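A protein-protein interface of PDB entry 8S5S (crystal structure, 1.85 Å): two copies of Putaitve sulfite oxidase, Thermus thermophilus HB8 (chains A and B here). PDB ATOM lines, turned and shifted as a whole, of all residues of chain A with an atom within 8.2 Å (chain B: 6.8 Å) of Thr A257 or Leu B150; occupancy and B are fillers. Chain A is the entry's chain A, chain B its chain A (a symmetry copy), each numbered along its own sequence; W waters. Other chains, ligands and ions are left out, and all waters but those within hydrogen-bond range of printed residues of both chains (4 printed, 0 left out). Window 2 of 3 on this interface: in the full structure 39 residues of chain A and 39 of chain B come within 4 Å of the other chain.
Water W4 bridges OE2 of Glu A221 (2.7 Å) and ND2 of Asn B238 (2.9 Å). Water W1 bridges the backbone carbonyl oxygen of Asn B238 (2.7 Å) and the guanidinium group of Arg A260 (3.5 Å). Water W2 lies within hydrogen-bond range of OD1 of Asn B238 (3.0 Å) and O of Ile A236 (3.4 Å). Water W3 lies within hydrogen-bond range of N of Asn B238 (3.3 Å) and N of Asn A238 (3.3 Å).
The side-chain hydroxyl of Ser A255 is in hydrogen-bond range of the backbone NH of Thr A257, at 3.1 Å. The backbone NH (N) of Leu A244 lies within hydrogen-bond range of the backbone carbonyl oxygen (O) of Pro A234. The side-chain hydroxyl (OG) of Ser A259 lies within hydrogen-bond range of the backbone carbonyl oxygen (O) of Ser A255. NE of Arg A232 sits at hydrogen-bond distance from OG of Ser A259, at 2.9 Å. N of Ile B171 lies within hydrogen-bond range of O of Leu B150, at 2.9 Å. O of Thr B218 lies within hydrogen-bond range of N of Leu B150 (2.9 Å).
The side-chain amide nitrogen (ND2) of Asn B238 is in hydrogen-bond range of the backbone carbonyl oxygen (O) of Ser A259, 3.5 Å away.
Asn B238 touches its own counterpart, Asn A238. Of the 8 pairs that touch across the chains among the printed residues, 1 has its exchanged pair printed and touching as well.
Printed residues of chain B within 4 Å of Thr A257: Leu B150 (3.7 Å). Of the printed residues of chain A, Leu B150 touches Thr A257 (3.7 Å). No residue of chain A comes within 4 Å of Ala B149. Printed residues of chain B within 4 Å of Ile A236: Pro B170 (3.8 Å) and His B172 (3.4 Å). Of the printed residues of chain B, Arg A260 touches Asn B238 (3.3 Å). Glu A221 touches none of the printed residues of chain B. Lys B148 touches none of the printed residues of chain A. The nearest printed residue of chain A that does not touch His B172 is Ala A235 (6.4 Å).
Printed residues of chain B that touch a printed residue of chain A: Leu B150, Pro B170, His B172 and Asn B238. Of the 18 printed residues of chain A, 7 touch a printed residue of chain B. Among the printed residues, 8 pairs touch across the chains.
Among the printed residues, merely in contact across the chains: Arg A260 with Asn B238 (3.3 Å), Pro A237 with Asn B238 (3.4 Å), Ile A236 with His B172 (3.4 Å), Leu A244 with His B172 (3.7 Å), Thr A257 with Leu B150 (3.7 Å), Ile A236 with Pro B170 (3.8 Å) and Asn A238 with Asn B238 (3.9 Å).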
ATOM      1  N   GLU A 221       8.726  17.180  30.555  1.00  0.00           N
ATOM      2  CA  GLU A 221       7.467  17.896  30.745  1.00  0.00           C
ATOM      3  C   GLU A 221       6.313  17.117  30.085  1.00  0.00           C
ATOM      4  O   GLU A 221       6.437  16.648  28.963  1.00  0.00           O
ATOM      5  CB  GLU A 221       7.521  19.229  30.020  1.00  0.00           C
ATOM      6  CG  GLU A 221       8.444  20.279  30.641  1.00  0.00           C
ATOM      7  CD  GLU A 221       8.259  21.639  29.973  1.00  0.00           C
ATOM      8  OE1 GLU A 221       7.142  22.242  30.055  1.00  0.00           O
ATOM      9  OE2 GLU A 221       9.192  22.097  29.292  1.00  0.00           O
ATOM     10  N   MET A 228       1.897  23.073  27.259  1.00  0.00           N
ATOM     11  CA  MET A 228       2.494  23.545  26.025  1.00  0.00           C
ATOM     12  C   MET A 228       1.378  23.483  24.994  1.00  0.00           C
ATOM     13  O   MET A 228       0.868  22.382  24.719  1.00  0.00           O
ATOM     14  CB  MET A 228       3.659  22.637  25.603  1.00  0.00           C
ATOM     15  CG  MET A 228       4.705  23.293  24.686  1.00  0.00           C
ATOM     16  SD  MET A 228       4.080  23.935  23.124  1.00  0.00           S
ATOM     17  CE  MET A 228       3.769  22.332  22.375  1.00  0.00           C
ATOM     18  N   ARG A 232       3.220  29.529  29.174  1.00  0.00           N
ATOM     19  CA  ARG A 232       4.618  29.725  28.762  1.00  0.00           C
ATOM     20  C   ARG A 232       4.883  31.126  28.234  1.00  0.00           C
ATOM     21  O   ARG A 232       3.995  31.833  27.728  1.00  0.00           O
ATOM     22  CB  ARG A 232       5.022  28.723  27.673  1.00  0.00           C
ATOM     23  CG  ARG A 232       4.827  27.242  27.961  1.00  0.00           C
ATOM     24  CD  ARG A 232       5.262  26.349  26.822  1.00  0.00           C
ATOM     25  NE  ARG A 232       6.671  25.944  26.879  1.00  0.00           N
ATOM     26  CZ  ARG A 232       7.168  24.986  27.596  1.00  0.00           C
ATOM     27  NH1 ARG A 232       6.380  24.197  28.298  1.00  0.00           N
ATOM     28  NH2 ARG A 232       8.493  24.842  27.668  1.00  0.00           N
ATOM     29  N   PRO A 234       8.068  33.343  25.862  1.00  0.00           N
ATOM     30  CA  PRO A 234       9.196  33.143  24.954  1.00  0.00           C
ATOM     31  C   PRO A 234      10.503  33.156  25.745  1.00  0.00           C
ATOM     32  O   PRO A 234      10.636  33.975  26.664  1.00  0.00           O
ATOM     33  CB  PRO A 234       9.098  34.356  24.061  1.00  0.00           C
ATOM     34  CG  PRO A 234       7.607  34.609  23.986  1.00  0.00           C
ATOM     35  CD  PRO A 234       7.231  34.501  25.468  1.00  0.00           C
ATOM     36  N   ALA A 235      11.446  32.323  25.331  1.00  0.00           N
ATOM     37  CA  ALA A 235      12.698  32.190  26.065  1.00  0.00           C
ATOM     38  C   ALA A 235      13.781  31.586  25.199  1.00  0.00           C
ATOM     39  O   ALA A 235      13.456  30.987  24.191  1.00  0.00           O
ATOM     40  CB  ALA A 235      12.463  31.280  27.246  1.00  0.00           C
ATOM     41  N   ILE A 236      15.044  31.703  25.666  1.00  0.00           N
ATOM     42  CA  ILE A 236      16.158  30.935  25.119  1.00  0.00           C
ATOM     43  C   ILE A 236      16.448  29.857  26.153  1.00  0.00           C
ATOM     44  O   ILE A 236      16.819  30.182  27.273  1.00  0.00           O
ATOM     45  CB  ILE A 236      17.410  31.786  24.863  1.00  0.00           C
ATOM     46  CG1 ILE A 236      17.145  32.992  23.980  1.00  0.00           C
ATOM     47  CG2 ILE A 236      18.532  30.928  24.284  1.00  0.00           C
ATOM     48  CD1 ILE A 236      18.336  33.916  23.839  1.00  0.00           C
ATOM     49  N   PRO A 237      16.108  28.584  25.913  1.00  0.00           N
ATOM     50  CA  PRO A 237      16.165  27.581  26.977  1.00  0.00           C
ATOM     51  C   PRO A 237      17.577  27.463  27.548  1.00  0.00           C
ATOM     52  O   PRO A 237      18.536  27.435  26.805  1.00  0.00           O
ATOM     53  CB  PRO A 237      15.681  26.313  26.286  1.00  0.00           C
ATOM     54  CG  PRO A 237      14.658  26.909  25.282  1.00  0.00           C
ATOM     55  CD  PRO A 237      15.489  28.061  24.688  1.00  0.00           C
ATOM     56  N   ASN A 238      17.639  27.503  28.873  1.00  0.00           N
ATOM     57  CA  ASN A 238      18.861  27.314  29.649  1.00  0.00           C
ATOM     58  C   ASN A 238      19.903  28.406  29.441  1.00  0.00           C
ATOM     59  O   ASN A 238      21.076  28.181  29.708  1.00  0.00           O
ATOM     60  CB  ASN A 238      19.437  25.925  29.419  1.00  0.00           C
ATOM     61  CG  ASN A 238      19.891  25.317  30.729  1.00  0.00           C
ATOM     62  OD1 ASN A 238      19.598  25.804  31.848  1.00  0.00           O
ATOM     63  ND2 ASN A 238      20.627  24.225  30.600  1.00  0.00           N
ATOM     64  N   LEU A 244      12.680  36.136  26.447  1.00  0.00           N
ATOM     65  CA  LEU A 244      13.131  36.719  25.198  1.00  0.00           C
ATOM     66  C   LEU A 244      12.064  37.712  24.737  1.00  0.00           C
ATOM     67  O   LEU A 244      10.990  37.307  24.309  1.00  0.00           O
ATOM     68  CB  LEU A 244      13.319  35.564  24.233  1.00  0.00           C
ATOM     69  CG  LEU A 244      13.986  35.896  22.917  1.00  0.00           C
ATOM     70  CD1 LEU A 244      15.427  36.337  23.266  1.00  0.00           C
ATOM     71  CD2 LEU A 244      13.879  34.670  22.000  1.00  0.00           C
ATOM     72  N   TYR A 252       3.109  34.352  18.701  1.00  0.00           N
ATOM     73  CA  TYR A 252       4.384  33.648  18.796  1.00  0.00           C
ATOM     74  C   TYR A 252       4.194  32.145  18.635  1.00  0.00           C
ATOM     75  O   TYR A 252       3.266  31.561  19.216  1.00  0.00           O
ATOM     76  CB  TYR A 252       4.964  34.005  20.166  1.00  0.00           C
ATOM     77  CG  TYR A 252       6.351  33.442  20.460  1.00  0.00           C
ATOM     78  CD1 TYR A 252       7.471  34.119  20.042  1.00  0.00           C
ATOM     79  CD2 TYR A 252       6.535  32.235  21.131  1.00  0.00           C
ATOM     80  CE1 TYR A 252       8.738  33.623  20.253  1.00  0.00           C
ATOM     81  CE2 TYR A 252       7.809  31.754  21.420  1.00  0.00           C
ATOM     82  CZ  TYR A 252       8.913  32.461  20.981  1.00  0.00           C
ATOM     83  OH  TYR A 252      10.204  32.108  21.159  1.00  0.00           O
ATOM     84  N   PRO A 253       5.075  31.436  17.870  1.00  0.00           N
ATOM     85  CA  PRO A 253       4.863  30.005  17.623  1.00  0.00           C
ATOM     86  C   PRO A 253       5.490  29.167  18.743  1.00  0.00           C
ATOM     87  O   PRO A 253       6.541  28.549  18.542  1.00  0.00           O
ATOM     88  CB  PRO A 253       5.582  29.814  16.273  1.00  0.00           C
ATOM     89  CG  PRO A 253       6.790  30.752  16.394  1.00  0.00           C
ATOM     90  CD  PRO A 253       6.247  31.975  17.136  1.00  0.00           C
ATOM     91  N   TYR A 254       4.821  29.143  19.897  1.00  0.00           N
ATOM     92  CA  TYR A 254       5.281  28.441  21.092  1.00  0.00           C
ATOM     93  C   TYR A 254       5.603  26.994  20.797  1.00  0.00           C
ATOM     94  O   TYR A 254       4.822  26.260  20.168  1.00  0.00           O
ATOM     95  CB  TYR A 254       4.273  28.442  22.240  1.00  0.00           C
ATOM     96  CG  TYR A 254       4.126  29.807  22.863  1.00  0.00           C
ATOM     97  CD1 TYR A 254       3.229  30.757  22.362  1.00  0.00           C
ATOM     98  CD2 TYR A 254       4.873  30.154  23.965  1.00  0.00           C
ATOM     99  CE1 TYR A 254       3.164  32.028  22.897  1.00  0.00           C
ATOM    100  CE2 TYR A 254       4.822  31.423  24.503  1.00  0.00           C
ATOM    101  CZ  TYR A 254       3.930  32.352  24.003  1.00  0.00           C
ATOM    102  OH  TYR A 254       3.913  33.580  24.537  1.00  0.00           O
ATOM    103  N   SER A 255       6.781  26.562  21.284  1.00  0.00           N
ATOM    104  CA  SER A 255       7.147  25.169  21.305  1.00  0.00           C
ATOM    105  C   SER A 255       7.887  24.900  22.605  1.00  0.00           C
ATOM    106  O   SER A 255       8.216  25.842  23.320  1.00  0.00           O
ATOM    107  CB  SER A 255       8.051  24.776  20.166  1.00  0.00           C
ATOM    108  OG  SER A 255       9.319  25.373  20.333  1.00  0.00           O
ATOM    109  N   PHE A 256       8.195  23.634  22.875  1.00  0.00           N
ATOM    110  CA  PHE A 256       9.057  23.308  24.025  1.00  0.00           C
ATOM    111  C   PHE A 256      10.456  23.897  23.926  1.00  0.00           C
ATOM    112  O   PHE A 256      11.149  23.998  24.955  1.00  0.00           O
ATOM    113  CB  PHE A 256       9.219  21.817  24.287  1.00  0.00           C
ATOM    114  CG  PHE A 256       7.980  21.166  24.869  1.00  0.00           C
ATOM    115  CD1 PHE A 256       7.645  21.376  26.205  1.00  0.00           C
ATOM    116  CD2 PHE A 256       7.182  20.314  24.095  1.00  0.00           C
ATOM    117  CE1 PHE A 256       6.519  20.797  26.752  1.00  0.00           C
ATOM    118  CE2 PHE A 256       6.060  19.713  24.660  1.00  0.00           C
ATOM    119  CZ  PHE A 256       5.715  19.984  25.968  1.00  0.00           C
ATOM    120  N   THR A 257      10.903  24.269  22.728  1.00  0.00           N
ATOM    121  CA  THR A 257      12.314  24.623  22.567  1.00  0.00           C
ATOM    122  C   THR A 257      12.513  26.115  22.339  1.00  0.00           C
ATOM    123  O   THR A 257      13.642  26.548  22.137  1.00  0.00           O
ATOM    124  CB  THR A 257      12.865  23.789  21.415  1.00  0.00           C
ATOM    125  OG1 THR A 257      12.133  24.085  20.238  1.00  0.00           O
ATOM    126  CG2 THR A 257      12.621  22.308  21.632  1.00  0.00           C
ATOM    127  N   ASN A 258      11.427  26.923  22.384  1.00  0.00           N
ATOM    128  CA  ASN A 258      11.547  28.362  22.239  1.00  0.00           C
ATOM    129  C   ASN A 258      10.813  29.121  23.336  1.00  0.00           C
ATOM    130  O   ASN A 258      10.596  30.331  23.236  1.00  0.00           O
ATOM    131  CB  ASN A 258      11.149  28.799  20.837  1.00  0.00           C
ATOM    132  CG  ASN A 258       9.667  28.701  20.649  1.00  0.00           C
ATOM    133  OD1 ASN A 258       8.924  28.378  21.580  1.00  0.00           O
ATOM    134  ND2 ASN A 258       9.220  29.027  19.447  1.00  0.00           N
ATOM    135  N   SER A 259      10.473  28.432  24.409  1.00  0.00           N
ATOM    136  CA  SER A 259       9.712  29.084  25.431  1.00  0.00           C
ATOM    137  C   SER A 259       9.885  28.305  26.717  1.00  0.00           C
ATOM    138  O   SER A 259      10.177  27.127  26.662  1.00  0.00           O
ATOM    139  CB  SER A 259       8.238  29.176  25.019  1.00  0.00           C
ATOM    140  OG  SER A 259       7.669  27.882  24.914  1.00  0.00           O
ATOM    141  N   ARG A 260       9.511  28.929  27.844  1.00  0.00           N
ATOM    142  CA  ARG A 260       9.643  28.284  29.133  1.00  0.00           C
ATOM    143  C   ARG A 260       8.332  28.403  29.907  1.00  0.00           C
ATOM    144  O   ARG A 260       7.496  29.300  29.682  1.00  0.00           O
ATOM    145  CB  ARG A 260      10.825  28.888  29.914  1.00  0.00           C
ATOM    146  CG  ARG A 260      10.503  30.307  30.392  1.00  0.00           C
ATOM    147  CD  ARG A 260      11.486  30.901  31.404  1.00  0.00           C
ATOM    148  NE  ARG A 260      11.184  32.246  31.906  1.00  0.00           N
ATOM    149  CZ  ARG A 260      10.119  32.673  32.640  1.00  0.00           C
ATOM    150  NH1 ARG A 260       9.178  31.848  33.057  1.00  0.00           N
ATOM    151  NH2 ARG A 260       9.913  33.968  32.841  1.00  0.00           N
ATOM    152  N   LEU B  76      22.142  19.389  10.621  1.00  0.00           N
ATOM    153  CA  LEU B  76      20.737  19.471  10.256  1.00  0.00           C
ATOM    154  C   LEU B  76      20.519  20.653   9.339  1.00  0.00           C
ATOM    155  O   LEU B  76      19.901  21.640   9.729  1.00  0.00           O
ATOM    156  CB  LEU B  76      19.905  19.579  11.526  1.00  0.00           C
ATOM    157  CG  LEU B  76      20.009  18.376  12.470  1.00  0.00           C
ATOM    158  CD1 LEU B  76      19.302  18.595  13.797  1.00  0.00           C
ATOM    159  CD2 LEU B  76      19.422  17.159  11.792  1.00  0.00           C
ATOM    160  N   GLY B 146      17.258  22.519   9.190  1.00  0.00           N
ATOM    161  CA  GLY B 146      16.242  21.575   9.591  1.00  0.00           C
ATOM    162  C   GLY B 146      15.479  22.086  10.808  1.00  0.00           C
ATOM    163  O   GLY B 146      15.985  22.899  11.601  1.00  0.00           O
ATOM    164  N   GLU B 147      14.293  21.501  11.013  1.00  0.00           N
ATOM    165  CA  GLU B 147      13.381  21.927  12.061  1.00  0.00           C
ATOM    166  C   GLU B 147      13.943  21.546  13.424  1.00  0.00           C
ATOM    167  O   GLU B 147      13.682  22.198  14.431  1.00  0.00           O
ATOM    168  CB  GLU B 147      12.036  21.253  11.723  1.00  0.00           C
ATOM    169  CG  GLU B 147      10.804  22.063  12.099  1.00  0.00           C
ATOM    170  CD  GLU B 147       9.508  21.249  12.087  1.00  0.00           C
ATOM    171  OE1 GLU B 147       8.879  21.208  13.163  1.00  0.00           O
ATOM    172  OE2 GLU B 147       9.161  20.621  11.054  1.00  0.00           O
ATOM    173  N   LYS B 148      14.780  20.504  13.466  1.00  0.00           N
ATOM    174  CA  LYS B 148      15.377  20.066  14.722  1.00  0.00           C
ATOM    175  C   LYS B 148      16.713  20.753  15.017  1.00  0.00           C
ATOM    176  O   LYS B 148      17.415  20.379  15.938  1.00  0.00           O
ATOM    177  CB  LYS B 148      15.573  18.548  14.674  1.00  0.00           C
ATOM    178  CG  LYS B 148      14.241  17.796  14.696  1.00  0.00           C
ATOM    179  CD  LYS B 148      14.444  16.293  14.795  1.00  0.00           C
ATOM    180  CE  LYS B 148      13.303  15.631  15.495  1.00  0.00           C
ATOM    181  NZ  LYS B 148      13.591  14.204  15.674  1.00  0.00           N
ATOM    182  N   ALA B 149      17.102  21.752  14.238  1.00  0.00           N
ATOM    183  CA  ALA B 149      18.376  22.407  14.515  1.00  0.00           C
ATOM    184  C   ALA B 149      18.219  23.317  15.738  1.00  0.00           C
ATOM    185  O   ALA B 149      17.640  24.371  15.624  1.00  0.00           O
ATOM    186  CB  ALA B 149      18.771  23.200  13.313  1.00  0.00           C
ATOM    187  N   LEU B 150      18.676  22.906  16.911  1.00  0.00           N
ATOM    188  CA  LEU B 150      18.476  23.731  18.085  1.00  0.00           C
ATOM    189  C   LEU B 150      19.764  24.380  18.586  1.00  0.00           C
ATOM    190  O   LEU B 150      19.692  25.200  19.500  1.00  0.00           O
ATOM    191  CB  LEU B 150      17.869  22.775  19.101  1.00  0.00           C
ATOM    192  CG  LEU B 150      16.449  22.293  18.764  1.00  0.00           C
ATOM    193  CD1 LEU B 150      16.109  21.339  19.859  1.00  0.00           C
ATOM    194  CD2 LEU B 150      15.465  23.418  18.726  1.00  0.00           C
ATOM    195  N   TYR B 151      20.926  23.960  18.053  1.00  0.00           N
ATOM    196  CA  TYR B 151      22.224  24.419  18.507  1.00  0.00           C
ATOM    197  C   TYR B 151      23.077  24.654  17.282  1.00  0.00           C
ATOM    198  O   TYR B 151      22.927  23.971  16.267  1.00  0.00           O
ATOM    199  CB  TYR B 151      22.989  23.449  19.438  1.00  0.00           C
ATOM    200  CG  TYR B 151      22.172  23.228  20.693  1.00  0.00           C
ATOM    201  CD1 TYR B 151      21.165  22.250  20.730  1.00  0.00           C
ATOM    202  CD2 TYR B 151      22.308  24.063  21.791  1.00  0.00           C
ATOM    203  CE1 TYR B 151      20.367  22.117  21.853  1.00  0.00           C
ATOM    204  CE2 TYR B 151      21.512  23.934  22.915  1.00  0.00           C
ATOM    205  CZ  TYR B 151      20.523  22.968  22.931  1.00  0.00           C
ATOM    206  OH  TYR B 151      19.782  22.814  24.059  1.00  0.00           O
ATOM    207  N   ILE B 152      24.015  25.583  17.429  1.00  0.00           N
ATOM    208  CA  ILE B 152      25.153  25.701  16.543  1.00  0.00           C
ATOM    209  C   ILE B 152      26.352  25.116  17.282  1.00  0.00           C
ATOM    210  O   ILE B 152      26.674  25.561  18.377  1.00  0.00           O
ATOM    211  CB  ILE B 152      25.413  27.175  16.168  1.00  0.00           C
ATOM    212  CG1 ILE B 152      24.148  27.872  15.650  1.00  0.00           C
ATOM    213  CG2 ILE B 152      26.581  27.268  15.196  1.00  0.00           C
ATOM    214  CD1 ILE B 152      24.341  29.356  15.405  1.00  0.00           C
ATOM    215  N   VAL B 169      26.173  26.504  21.119  1.00  0.00           N
ATOM    216  CA  VAL B 169      25.388  27.641  21.551  1.00  0.00           C
ATOM    217  C   VAL B 169      23.975  27.437  20.977  1.00  0.00           C
ATOM    218  O   VAL B 169      23.748  26.710  19.987  1.00  0.00           O
ATOM    219  CB  VAL B 169      25.996  28.989  21.108  1.00  0.00           C
ATOM    220  CG1 VAL B 169      27.382  29.237  21.694  1.00  0.00           C
ATOM    221  CG2 VAL B 169      26.058  29.116  19.595  1.00  0.00           C
ATOM    222  N   PRO B 170      22.968  28.083  21.579  1.00  0.00           N
ATOM    223  CA  PRO B 170      21.584  27.971  21.091  1.00  0.00           C
ATOM    224  C   PRO B 170      21.415  28.549  19.691  1.00  0.00           C
ATOM    225  O   PRO B 170      22.121  29.484  19.287  1.00  0.00           O
ATOM    226  CB  PRO B 170      20.747  28.737  22.104  1.00  0.00           C
ATOM    227  CG  PRO B 170      21.664  29.136  23.187  1.00  0.00           C
ATOM    228  CD  PRO B 170      23.101  28.966  22.730  1.00  0.00           C
ATOM    229  N   ILE B 171      20.484  27.966  18.944  1.00  0.00           N
ATOM    230  CA  ILE B 171      20.232  28.377  17.577  1.00  0.00           C
ATOM    231  C   ILE B 171      19.777  29.848  17.534  1.00  0.00           C
ATOM    232  O   ILE B 171      19.980  30.535  16.535  1.00  0.00           O
ATOM    233  CB  ILE B 171      19.229  27.434  16.878  1.00  0.00           C
ATOM    234  CG1 ILE B 171      19.238  27.611  15.360  1.00  0.00           C
ATOM    235  CG2 ILE B 171      17.830  27.582  17.470  1.00  0.00           C
ATOM    236  CD1 ILE B 171      20.591  27.341  14.716  1.00  0.00           C
ATOM    237  N   HIS B 172      19.225  30.376  18.610  1.00  0.00           N
ATOM    238  CA  HIS B 172      18.947  31.802  18.655  1.00  0.00           C
ATOM    239  C   HIS B 172      20.187  32.638  18.283  1.00  0.00           C
ATOM    240  O   HIS B 172      20.065  33.708  17.728  1.00  0.00           O
ATOM    241  CB  HIS B 172      18.415  32.191  20.020  1.00  0.00           C
ATOM    242  CG  HIS B 172      17.971  33.611  20.094  1.00  0.00           C
ATOM    243  ND1 HIS B 172      18.840  34.596  20.520  1.00  0.00           N
ATOM    244  CD2 HIS B 172      16.786  34.209  19.800  1.00  0.00           C
ATOM    245  CE1 HIS B 172      18.222  35.760  20.448  1.00  0.00           C
ATOM    246  NE2 HIS B 172      16.960  35.553  20.015  1.00  0.00           N
ATOM    247  N   PHE B 217      24.881  22.165  12.636  1.00  0.00           N
ATOM    248  CA  PHE B 217      23.619  22.426  13.326  1.00  0.00           C
ATOM    249  C   PHE B 217      23.130  21.128  13.960  1.00  0.00           C
ATOM    250  O   PHE B 217      22.922  20.158  13.262  1.00  0.00           O
ATOM    251  CB  PHE B 217      22.690  23.055  12.292  1.00  0.00           C
ATOM    252  CG  PHE B 217      23.237  24.365  11.770  1.00  0.00           C
ATOM    253  CD1 PHE B 217      23.000  25.560  12.446  1.00  0.00           C
ATOM    254  CD2 PHE B 217      24.043  24.395  10.643  1.00  0.00           C
ATOM    255  CE1 PHE B 217      23.574  26.745  11.997  1.00  0.00           C
ATOM    256  CE2 PHE B 217      24.562  25.587  10.176  1.00  0.00           C
ATOM    257  CZ  PHE B 217      24.345  26.763  10.862  1.00  0.00           C
ATOM    258  N   THR B 218      22.956  21.126  15.279  1.00  0.00           N
ATOM    259  CA  THR B 218      22.744  19.908  16.026  1.00  0.00           C
ATOM    260  C   THR B 218      21.469  20.066  16.837  1.00  0.00           C
ATOM    261  O   THR B 218      21.023  21.179  17.156  1.00  0.00           O
ATOM    262  CB  THR B 218      23.929  19.536  16.927  1.00  0.00           C
ATOM    263  OG1 THR B 218      24.166  20.570  17.862  1.00  0.00           O
ATOM    264  CG2 THR B 218      25.224  19.328  16.169  1.00  0.00           C
ATOM    265  N   GLU B 219      20.913  18.911  17.191  1.00  0.00           N
ATOM    266  CA  GLU B 219      19.668  18.864  17.952  1.00  0.00           C
ATOM    267  C   GLU B 219      19.966  18.968  19.448  1.00  0.00           C
ATOM    268  O   GLU B 219      19.119  19.370  20.223  1.00  0.00           O
ATOM    269  CB  GLU B 219      18.962  17.530  17.705  1.00  0.00           C
ATOM    270  CG  GLU B 219      17.543  17.501  18.277  1.00  0.00           C
ATOM    271  CD  GLU B 219      16.755  16.208  17.975  1.00  0.00           C
ATOM    272  OE1 GLU B 219      17.290  15.295  17.312  1.00  0.00           O
ATOM    273  OE2 GLU B 219      15.588  16.124  18.405  1.00  0.00           O
ATOM    274  N   ALA B 220      21.204  18.648  19.855  1.00  0.00           N
ATOM    275  CA  ALA B 220      21.617  18.683  21.255  1.00  0.00           C
ATOM    276  C   ALA B 220      22.969  19.379  21.421  1.00  0.00           C
ATOM    277  O   ALA B 220      23.716  19.523  20.463  1.00  0.00           O
ATOM    278  CB  ALA B 220      21.732  17.261  21.783  1.00  0.00           C
ATOM    279  N   ASN B 238      15.725  25.950  32.373  1.00  0.00           N
ATOM    280  CA  ASN B 238      14.543  26.611  31.830  1.00  0.00           C
ATOM    281  C   ASN B 238      13.648  27.248  32.885  1.00  0.00           C
ATOM    282  O   ASN B 238      12.475  27.481  32.621  1.00  0.00           O
ATOM    283  CB  ASN B 238      13.771  25.671  30.917  1.00  0.00           C
ATOM    284  CG  ASN B 238      13.326  26.394  29.664  1.00  0.00           C
ATOM    285  OD1 ASN B 238      13.757  27.528  29.339  1.00  0.00           O
ATOM    286  ND2 ASN B 238      12.442  25.735  28.935  1.00  0.00           N
HETATM  287  O   HOH W   1      10.323  28.652  33.764  1.00  0.00           O
HETATM  288  O   HOH W   2      14.864  30.180  30.107  1.00  0.00           O
HETATM  289  O   HOH W   3      16.874  28.986  31.731  1.00  0.00           O
HETATM  290  O   HOH W   4      11.385  23.334  30.239  1.00  0.00           O
